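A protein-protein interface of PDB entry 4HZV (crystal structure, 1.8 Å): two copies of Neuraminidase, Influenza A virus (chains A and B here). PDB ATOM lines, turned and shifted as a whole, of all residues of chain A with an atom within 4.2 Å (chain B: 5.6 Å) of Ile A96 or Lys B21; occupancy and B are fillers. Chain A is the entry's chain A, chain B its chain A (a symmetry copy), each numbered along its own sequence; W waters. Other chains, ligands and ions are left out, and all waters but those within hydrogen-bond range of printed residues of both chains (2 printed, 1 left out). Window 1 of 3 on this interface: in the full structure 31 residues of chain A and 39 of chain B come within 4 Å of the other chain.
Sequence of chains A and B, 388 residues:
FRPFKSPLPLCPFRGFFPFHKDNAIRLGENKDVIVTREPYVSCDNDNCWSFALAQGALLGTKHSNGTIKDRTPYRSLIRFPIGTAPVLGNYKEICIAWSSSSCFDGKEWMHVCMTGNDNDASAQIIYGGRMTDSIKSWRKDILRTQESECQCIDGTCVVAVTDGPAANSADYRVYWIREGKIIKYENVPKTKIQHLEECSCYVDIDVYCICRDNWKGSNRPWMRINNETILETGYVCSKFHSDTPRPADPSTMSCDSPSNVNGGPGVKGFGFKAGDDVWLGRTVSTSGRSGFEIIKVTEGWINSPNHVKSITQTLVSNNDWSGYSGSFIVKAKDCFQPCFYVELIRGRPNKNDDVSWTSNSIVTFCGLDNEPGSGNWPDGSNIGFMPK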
ATOM      1  N   PRO A  73      21.369  15.053 -23.559  1.00  0.00           N
ATOM      2  CA  PRO A  73      20.719  16.371 -23.619  1.00  0.00           C
ATOM      3  C   PRO A  73      21.559  17.442 -22.930  1.00  0.00           C
ATOM      4  O   PRO A  73      21.275  18.636 -23.067  1.00  0.00           O
ATOM      5  CB  PRO A  73      19.423  16.164 -22.817  1.00  0.00           C
ATOM      6  CG  PRO A  73      19.230  14.679 -22.742  1.00  0.00           C
ATOM      7  CD  PRO A  73      20.610  14.094 -22.740  1.00  0.00           C
ATOM      8  N   TYR A  74      22.577  17.009 -22.192  1.00  0.00           N
ATOM      9  CA  TYR A  74      23.368  17.902 -21.353  1.00  0.00           C
ATOM     10  C   TYR A  74      24.629  18.365 -22.054  1.00  0.00           C
ATOM     11  O   TYR A  74      25.482  19.010 -21.443  1.00  0.00           O
ATOM     12  CB  TYR A  74      23.695  17.214 -20.026  1.00  0.00           C
ATOM     13  CG  TYR A  74      22.493  16.452 -19.518  1.00  0.00           C
ATOM     14  CD1 TYR A  74      21.285  17.098 -19.314  1.00  0.00           C
ATOM     15  CD2 TYR A  74      22.545  15.080 -19.309  1.00  0.00           C
ATOM     16  CE1 TYR A  74      20.172  16.410 -18.887  1.00  0.00           C
ATOM     17  CE2 TYR A  74      21.431  14.382 -18.876  1.00  0.00           C
ATOM     18  CZ  TYR A  74      20.250  15.053 -18.673  1.00  0.00           C
ATOM     19  OH  TYR A  74      19.134  14.378 -18.237  1.00  0.00           O
ATOM     20  N   ARG A  75      24.742  18.029 -23.336  1.00  0.00           N
ATOM     21  CA  ARG A  75      25.860  18.489 -24.144  1.00  0.00           C
ATOM     22  C   ARG A  75      25.490  19.775 -24.876  1.00  0.00           C
ATOM     23  O   ARG A  75      24.393  19.900 -25.425  1.00  0.00           O
ATOM     24  CB  ARG A  75      26.318  17.411 -25.136  1.00  0.00           C
ATOM     25  CG  ARG A  75      26.714  16.093 -24.470  1.00  0.00           C
ATOM     26  CD  ARG A  75      27.671  15.270 -25.341  1.00  0.00           C
ATOM     27  NE  ARG A  75      29.036  15.811 -25.328  1.00  0.00           N
ATOM     28  CZ  ARG A  75      30.061  15.273 -25.985  1.00  0.00           C
ATOM     29  NH1 ARG A  75      29.886  14.174 -26.713  1.00  0.00           N
ATOM     30  NH2 ARG A  75      31.270  15.831 -25.914  1.00  0.00           N
ATOM     31  N   SER A  76      26.413  20.733 -24.849  1.00  0.00           N
ATOM     32  CA  SER A  76      26.270  21.995 -25.555  1.00  0.00           C
ATOM     33  C   SER A  76      27.562  22.272 -26.302  1.00  0.00           C
ATOM     34  O   SER A  76      28.644  21.966 -25.809  1.00  0.00           O
ATOM     35  CB  SER A  76      26.052  23.152 -24.567  1.00  0.00           C
ATOM     36  OG  SER A  76      24.767  23.115 -23.968  1.00  0.00           O
ATOM     37  N   GLU A  93      28.172  29.524 -24.045  1.00  0.00           N
ATOM     38  CA  GLU A  93      27.401  28.399 -24.568  1.00  0.00           C
ATOM     39  C   GLU A  93      26.769  28.799 -25.898  1.00  0.00           C
ATOM     40  O   GLU A  93      25.980  29.738 -25.957  1.00  0.00           O
ATOM     41  CB  GLU A  93      26.334  27.922 -23.572  1.00  0.00           C
ATOM     42  CG  GLU A  93      25.750  26.526 -23.913  1.00  0.00           C
ATOM     43  CD  GLU A  93      24.277  26.553 -24.310  1.00  0.00           C
ATOM     44  OE1 GLU A  93      23.737  27.651 -24.547  1.00  0.00           O
ATOM     45  OE2 GLU A  93      23.652  25.468 -24.392  1.00  0.00           O
ATOM     46  N   CYS A  95      25.080  26.655 -28.285  1.00  0.00           N
ATOM     47  CA  CYS A  95      23.806  26.000 -28.550  1.00  0.00           C
ATOM     48  C   CYS A  95      23.813  24.612 -27.932  1.00  0.00           C
ATOM     49  O   CYS A  95      24.873  24.066 -27.619  1.00  0.00           O
ATOM     50  CB  CYS A  95      23.611  25.861 -30.054  1.00  0.00           C
ATOM     51  SG  CYS A  95      24.960  24.909 -30.840  1.00  0.00           S
ATOM     52  N   ILE A  96      22.630  24.039 -27.755  1.00  0.00           N
ATOM     53  CA  ILE A  96      22.535  22.652 -27.333  1.00  0.00           C
ATOM     54  C   ILE A  96      22.970  21.793 -28.501  1.00  0.00           C
ATOM     55  O   ILE A  96      22.439  21.930 -29.605  1.00  0.00           O
ATOM     56  CB  ILE A  96      21.097  22.284 -26.943  1.00  0.00           C
ATOM     57  CG1 ILE A  96      20.602  23.207 -25.824  1.00  0.00           C
ATOM     58  CG2 ILE A  96      21.026  20.817 -26.535  1.00  0.00           C
ATOM     59  CD1 ILE A  96      19.078  23.267 -25.694  1.00  0.00           C
ATOM     60  N   ALA A  97      23.949  20.919 -28.273  1.00  0.00           N
ATOM     61  CA  ALA A  97      24.452  20.087 -29.360  1.00  0.00           C
ATOM     62  C   ALA A  97      25.250  18.880 -28.889  1.00  0.00           C
ATOM     63  O   ALA A  97      26.077  18.991 -27.976  1.00  0.00           O
ATOM     64  CB  ALA A  97      25.299  20.934 -30.320  1.00  0.00           C
ATOM     65  N   CYS A 113      24.011  22.748 -34.988  1.00  0.00           N
ATOM     66  CA  CYS A 113      23.930  22.077 -33.696  1.00  0.00           C
ATOM     67  C   CYS A 113      22.892  20.961 -33.718  1.00  0.00           C
ATOM     68  O   CYS A 113      21.701  21.232 -33.824  1.00  0.00           O
ATOM     69  CB  CYS A 113      23.525  23.098 -32.633  1.00  0.00           C
ATOM     70  SG  CYS A 113      24.419  24.672 -32.781  1.00  0.00           S
ATOM     71  N   THR A 115      20.824  17.957 -31.829  1.00  0.00           N
ATOM     72  CA  THR A 115      20.461  17.402 -30.532  1.00  0.00           C
ATOM     73  C   THR A 115      19.124  16.670 -30.608  1.00  0.00           C
ATOM     74  O   THR A 115      18.487  16.634 -31.665  1.00  0.00           O
ATOM     75  CB  THR A 115      20.445  18.483 -29.425  1.00  0.00           C
ATOM     76  OG1 THR A 115      20.271  17.865 -28.144  1.00  0.00           O
ATOM     77  CG2 THR A 115      19.324  19.468 -29.670  1.00  0.00           C
ATOM     78  N   PRO B  18      15.290  23.302 -29.796  1.00  0.00           N
ATOM     79  CA  PRO B  18      16.205  23.517 -28.667  1.00  0.00           C
ATOM     80  C   PRO B  18      17.297  24.530 -29.000  1.00  0.00           C
ATOM     81  O   PRO B  18      17.970  24.425 -30.020  1.00  0.00           O
ATOM     82  CB  PRO B  18      16.814  22.131 -28.442  1.00  0.00           C
ATOM     83  CG  PRO B  18      16.702  21.456 -29.771  1.00  0.00           C
ATOM     84  CD  PRO B  18      15.413  21.944 -30.353  1.00  0.00           C
ATOM     85  N   PHE B  19      17.471  25.497 -28.108  1.00  0.00           N
ATOM     86  CA  PHE B  19      18.324  26.656 -28.360  1.00  0.00           C
ATOM     87  C   PHE B  19      19.559  26.591 -27.461  1.00  0.00           C
ATOM     88  O   PHE B  19      20.603  26.057 -27.862  1.00  0.00           O
ATOM     89  CB  PHE B  19      17.499  27.919 -28.075  1.00  0.00           C
ATOM     90  CG  PHE B  19      18.111  29.206 -28.579  1.00  0.00           C
ATOM     91  CD1 PHE B  19      19.059  29.215 -29.587  1.00  0.00           C
ATOM     92  CD2 PHE B  19      17.697  30.420 -28.045  1.00  0.00           C
ATOM     93  CE1 PHE B  19      19.603  30.412 -30.041  1.00  0.00           C
ATOM     94  CE2 PHE B  19      18.236  31.618 -28.494  1.00  0.00           C
ATOM     95  CZ  PHE B  19      19.185  31.612 -29.493  1.00  0.00           C
ATOM     96  N   HIS B  20      19.417  27.119 -26.243  1.00  0.00           N
ATOM     97  CA  HIS B  20      20.480  27.160 -25.237  1.00  0.00           C
ATOM     98  C   HIS B  20      20.060  26.392 -23.988  1.00  0.00           C
ATOM     99  O   HIS B  20      18.907  26.450 -23.588  1.00  0.00           O
ATOM    100  CB  HIS B  20      20.749  28.608 -24.805  1.00  0.00           C
ATOM    101  CG  HIS B  20      21.416  29.452 -25.848  1.00  0.00           C
ATOM    102  ND1 HIS B  20      22.787  29.510 -25.994  1.00  0.00           N
ATOM    103  CD2 HIS B  20      20.905  30.303 -26.768  1.00  0.00           C
ATOM    104  CE1 HIS B  20      23.089  30.346 -26.972  1.00  0.00           C
ATOM    105  NE2 HIS B  20      21.966  30.847 -27.454  1.00  0.00           N
ATOM    106  N   LYS B  21      21.007  25.709 -23.349  1.00  0.00           N
ATOM    107  CA  LYS B  21      20.738  25.021 -22.087  1.00  0.00           C
ATOM    108  C   LYS B  21      21.941  25.175 -21.177  1.00  0.00           C
ATOM    109  O   LYS B  21      23.067  24.932 -21.607  1.00  0.00           O
ATOM    110  CB  LYS B  21      20.459  23.529 -22.327  1.00  0.00           C
ATOM    111  CG  LYS B  21      20.072  22.751 -21.063  1.00  0.00           C
ATOM    112  CD  LYS B  21      19.852  21.255 -21.364  1.00  0.00           C
ATOM    113  CE  LYS B  21      19.158  20.550 -20.197  1.00  0.00           C
ATOM    114  NZ  LYS B  21      19.876  20.720 -18.902  1.00  0.00           N
ATOM    115  N   ASP B  22      21.728  25.574 -19.922  1.00  0.00           N
ATOM    116  CA  ASP B  22      22.879  25.889 -19.072  1.00  0.00           C
ATOM    117  C   ASP B  22      23.390  24.764 -18.170  1.00  0.00           C
ATOM    118  O   ASP B  22      24.561  24.756 -17.812  1.00  0.00           O
ATOM    119  CB  ASP B  22      22.718  27.227 -18.305  1.00  0.00           C
ATOM    120  CG  ASP B  22      21.559  27.229 -17.319  1.00  0.00           C
ATOM    121  OD1 ASP B  22      21.057  26.150 -16.951  1.00  0.00           O
ATOM    122  OD2 ASP B  22      21.161  28.340 -16.890  1.00  0.00           O
ATOM    123  N   ASN B  23      22.533  23.806 -17.830  1.00  0.00           N
ATOM    124  CA  ASN B  23      22.971  22.704 -16.981  1.00  0.00           C
ATOM    125  C   ASN B  23      23.557  23.248 -15.680  1.00  0.00           C
ATOM    126  O   ASN B  23      24.521  22.708 -15.140  1.00  0.00           O
ATOM    127  CB  ASN B  23      24.003  21.841 -17.724  1.00  0.00           C
ATOM    128  CG  ASN B  23      23.446  21.250 -19.012  1.00  0.00           C
ATOM    129  OD1 ASN B  23      23.866  21.606 -20.115  1.00  0.00           O
ATOM    130  ND2 ASN B  23      22.484  20.354 -18.874  1.00  0.00           N
ATOM    131  N   ARG B  26      23.893  20.804 -12.435  1.00  0.00           N
ATOM    132  CA  ARG B  26      24.990  19.867 -12.709  1.00  0.00           C
ATOM    133  C   ARG B  26      26.358  20.540 -12.539  1.00  0.00           C
ATOM    134  O   ARG B  26      27.253  20.009 -11.877  1.00  0.00           O
ATOM    135  CB  ARG B  26      24.873  19.291 -14.127  1.00  0.00           C
ATOM    136  CG  ARG B  26      23.669  18.370 -14.344  1.00  0.00           C
ATOM    137  CD  ARG B  26      23.483  18.000 -15.827  1.00  0.00           C
ATOM    138  NE  ARG B  26      24.699  17.474 -16.453  1.00  0.00           N
ATOM    139  CZ  ARG B  26      25.015  16.186 -16.532  1.00  0.00           C
ATOM    140  NH1 ARG B  26      26.144  15.815 -17.123  1.00  0.00           N
ATOM    141  NH2 ARG B  26      24.212  15.265 -16.020  1.00  0.00           N
ATOM    142  N   GLY B  83      22.726  30.549 -21.638  1.00  0.00           N
ATOM    143  CA  GLY B  83      23.188  29.177 -21.658  1.00  0.00           C
ATOM    144  C   GLY B  83      24.386  28.867 -20.771  1.00  0.00           C
ATOM    145  O   GLY B  83      24.810  27.709 -20.708  1.00  0.00           O
ATOM    146  N   THR B  84      24.948  29.874 -20.102  1.00  0.00           N
ATOM    147  CA  THR B  84      26.020  29.620 -19.132  1.00  0.00           C
ATOM    148  C   THR B  84      25.476  29.555 -17.705  1.00  0.00           C
ATOM    149  O   THR B  84      24.444  30.160 -17.385  1.00  0.00           O
ATOM    150  CB  THR B  84      27.169  30.682 -19.171  1.00  0.00           C
ATOM    151  OG1 THR B  84      26.688  31.949 -18.693  1.00  0.00           O
ATOM    152  CG2 THR B  84      27.754  30.827 -20.577  1.00  0.00           C
ATOM    153  N   LEU B 344      13.909  25.152 -14.641  1.00  0.00           N
ATOM    154  CA  LEU B 344      13.919  23.782 -14.153  1.00  0.00           C
ATOM    155  C   LEU B 344      14.337  23.811 -12.690  1.00  0.00           C
ATOM    156  O   LEU B 344      15.524  23.857 -12.369  1.00  0.00           O
ATOM    157  CB  LEU B 344      14.865  22.917 -14.999  1.00  0.00           C
ATOM    158  CG  LEU B 344      14.726  23.040 -16.525  1.00  0.00           C
ATOM    159  CD1 LEU B 344      15.829  22.287 -17.263  1.00  0.00           C
ATOM    160  CD2 LEU B 344      13.365  22.568 -17.003  1.00  0.00           C
ATOM    161  N   SER B 361      17.950  25.402 -13.129  1.00  0.00           N
ATOM    162  CA  SER B 361      18.699  25.584 -14.364  1.00  0.00           C
ATOM    163  C   SER B 361      17.735  26.141 -15.401  1.00  0.00           C
ATOM    164  O   SER B 361      16.568  26.383 -15.097  1.00  0.00           O
ATOM    165  CB  SER B 361      19.361  24.285 -14.841  1.00  0.00           C
ATOM    166  OG  SER B 361      18.401  23.294 -15.166  1.00  0.00           O
ATOM    167  N   ILE B 362      18.227  26.351 -16.614  1.00  0.00           N
ATOM    168  CA  ILE B 362      17.438  26.947 -17.678  1.00  0.00           C
ATOM    169  C   ILE B 362      17.548  26.143 -18.960  1.00  0.00           C
ATOM    170  O   ILE B 362      18.614  25.615 -19.290  1.00  0.00           O
ATOM    171  CB  ILE B 362      17.932  28.380 -17.983  1.00  0.00           C
ATOM    172  CG1 ILE B 362      17.892  29.241 -16.721  1.00  0.00           C
ATOM    173  CG2 ILE B 362      17.112  29.020 -19.099  1.00  0.00           C
ATOM    174  CD1 ILE B 362      18.478  30.618 -16.923  1.00  0.00           C
ATOM    175  N   VAL B 363      16.448  26.052 -19.696  1.00  0.00           N
ATOM    176  CA  VAL B 363      16.507  25.546 -21.059  1.00  0.00           C
ATOM    177  C   VAL B 363      15.647  26.453 -21.929  1.00  0.00           C
ATOM    178  O   VAL B 363      14.689  27.048 -21.445  1.00  0.00           O
ATOM    179  CB  VAL B 363      16.051  24.069 -21.152  1.00  0.00           C
ATOM    180  CG1 VAL B 363      14.560  23.932 -20.797  1.00  0.00           C
ATOM    181  CG2 VAL B 363      16.351  23.500 -22.531  1.00  0.00           C
ATOM    182  N   THR B 364      16.002  26.582 -23.200  1.00  0.00           N
ATOM    183  CA  THR B 364      15.304  27.509 -24.079  1.00  0.00           C
ATOM    184  C   THR B 364      15.025  26.895 -25.442  1.00  0.00           C
ATOM    185  O   THR B 364      15.760  26.015 -25.905  1.00  0.00           O
ATOM    186  CB  THR B 364      16.111  28.811 -24.278  1.00  0.00           C
ATOM    187  OG1 THR B 364      17.388  28.492 -24.843  1.00  0.00           O
ATOM    188  CG2 THR B 364      16.318  29.523 -22.955  1.00  0.00           C
ATOM    189  N   TRP B 377      14.980  17.435 -22.641  1.00  0.00           N
ATOM    190  CA  TRP B 377      16.050  18.298 -22.132  1.00  0.00           C
ATOM    191  C   TRP B 377      15.748  18.811 -20.731  1.00  0.00           C
ATOM    192  O   TRP B 377      15.469  20.000 -20.540  1.00  0.00           O
ATOM    193  CB  TRP B 377      16.274  19.476 -23.078  1.00  0.00           C
ATOM    194  CG  TRP B 377      16.673  19.073 -24.464  1.00  0.00           C
ATOM    195  CD1 TRP B 377      17.945  18.877 -24.932  1.00  0.00           C
ATOM    196  CD2 TRP B 377      15.796  18.818 -25.569  1.00  0.00           C
ATOM    197  NE1 TRP B 377      17.909  18.513 -26.258  1.00  0.00           N
ATOM    198  CE2 TRP B 377      16.601  18.473 -26.672  1.00  0.00           C
ATOM    199  CE3 TRP B 377      14.406  18.852 -25.730  1.00  0.00           C
ATOM    200  CZ2 TRP B 377      16.063  18.160 -27.921  1.00  0.00           C
ATOM    201  CZ3 TRP B 377      13.873  18.544 -26.970  1.00  0.00           C
ATOM    202  CH2 TRP B 377      14.700  18.198 -28.049  1.00  0.00           C
ATOM    203  N   PRO B 378      15.821  17.916 -19.735  1.00  0.00           N
ATOM    204  CA  PRO B 378      15.512  18.226 -18.338  1.00  0.00           C
ATOM    205  C   PRO B 378      16.744  18.759 -17.623  1.00  0.00           C
ATOM    206  O   PRO B 378      17.803  18.834 -18.238  1.00  0.00           O
ATOM    207  CB  PRO B 378      15.165  16.857 -17.772  1.00  0.00           C
ATOM    208  CG  PRO B 378      16.060  15.921 -18.527  1.00  0.00           C
ATOM    209  CD  PRO B 378      16.341  16.547 -19.880  1.00  0.00           C
ATOM    210  N   ASP B 379      16.610  19.106 -16.347  1.00  0.00           N
ATOM    211  CA  ASP B 379      17.732  19.640 -15.580  1.00  0.00           C
ATOM    212  C   ASP B 379      18.948  18.710 -15.635  1.00  0.00           C
ATOM    213  O   ASP B 379      20.074  19.146 -15.874  1.00  0.00           O
ATOM    214  CB  ASP B 379      17.332  19.862 -14.130  1.00  0.00           C
ATOM    215  CG  ASP B 379      18.519  20.172 -13.262  1.00  0.00           C
ATOM    216  OD1 ASP B 379      19.037  21.305 -13.357  1.00  0.00           O
ATOM    217  OD2 ASP B 379      18.956  19.276 -12.516  1.00  0.00           O
ATOM    218  N   GLY B 380      18.713  17.426 -15.396  1.00  0.00           N
ATOM    219  CA  GLY B 380      19.749  16.427 -15.573  1.00  0.00           C
ATOM    220  C   GLY B 380      20.657  16.187 -14.383  1.00  0.00           C
ATOM    221  O   GLY B 380      21.576  15.366 -14.469  1.00  0.00           O
HETATM  222  O   HOH W   1      20.582  23.433 -30.912  1.00  0.00           O
HETATM  223  O   HOH W   2      25.955  23.411 -21.150  1.00  0.00           O
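The backbone carbonyl oxygen (O) of Lys B21 lies within hydrogen-bond range of the side-chain hydroxyl (OG) of Ser A76 (3.4 Å). OE1 of Glu A93 lies within hydrogen-bond range of ND1 of His B20, at 2.5 Å. The backbone carbonyl oxygen of Phe B19 sits at hydrogen-bond distance from the backbone NH of Ile A96 (2.9 Å). OE2 of Glu A93 sits at hydrogen-bond distance from N of Lys B21, 2.9 Å away. OG1 of Thr A115 sits at hydrogen-bond distance from NE1 of Trp B377 (3.1 Å). OD1 of Asn B23 sits close to O of Tyr A74, 3.3 Å away.
N of His B20 is in hydrogen-bond range of OG1 of Thr B364 (2.8 Å). O of Asp B379 sits at hydrogen-bond distance from NZ of Lys B21 (3.4 Å). OE2 of Glu A93 lies within hydrogen-bond range of OG of Ser A76 (2.6 Å). The guanidinium group (NH2) of Arg B26 sits at hydrogen-bond distance from the backbone carbonyl oxygen (O) of Gly B380 (3.1 Å). SG of Cys A113 is disulfide-bonded to SG of Cys A95 (2.0 Å). The backbone NH (N) of Phe B19 lies within hydrogen-bond range of the backbone carbonyl oxygen (O) of Thr B364 (2.8 Å).
O of Pro A73 touches CD of Lys B21 (3.4 Å). Trp B377 touches Pro A73 (CD1 to CB, 3.7 Å). Lys B21 touches Tyr A74 (NZ to CD1, 3.9 Å). Glu A93 touches Gly B83 (CB to O, 3.3 Å). Thr B84 touches Glu A93. O of Phe B19 touches CA of Cys A95 (3.3 Å). Ile A96 touches Pro B18. C of His B20 touches CD1 of Ile A96, 3.7 Å away. CG1 of Ile A96 touches CB of Lys B21, at 3.5 Å. Pro B18 touches Thr A115.
Lys B21 touches just these residues of chain A: Pro A73 (3.4 Å), Tyr A74 (3.9 Å), Ser A76 (3.4 Å), Glu A93 (2.9 Å) and Ile A96 (3.5 Å). Printed residues of chain B within 4 Å of Tyr A74: Lys B21, Asn B23, Arg B26, Pro B378 and Gly B380. Of the printed residues of chain B, Ser A76 touches Lys B21. The nearest printed residue of chain B that does not touch Glu A93 is Phe B19 (4.7 Å).
Of the 10 printed residues of chain A, 7 touch a printed residue of chain B. Hydrophobic or aromatic side chains of chain A within 4 Å of the printed part of chain B: Pro A73, Tyr A74 and Ile A96. Hydrophobic or aromatic side chains of chain B within 4 Å of the printed part of chain A: Pro B18, His B20, Trp B377 and Pro B378. Along chain B the printed residues that touch a printed residue of chain A span positions 18 to 380. Among the printed residues, 20 pairs touch across the chains.
No position is printed for both chains. Of the 20 pairs that touch across the chains among the printed residues, none has its exchanged pair printed and touching as well.
Water W1 lies within hydrogen-bond range of O of Ile A96 (2.7 Å) and O of Pro B18 (2.9 Å). Water W2 lies within hydrogen-bond range of OD1 of Asn B23, OG of Ser A76 and O of Lys B21.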
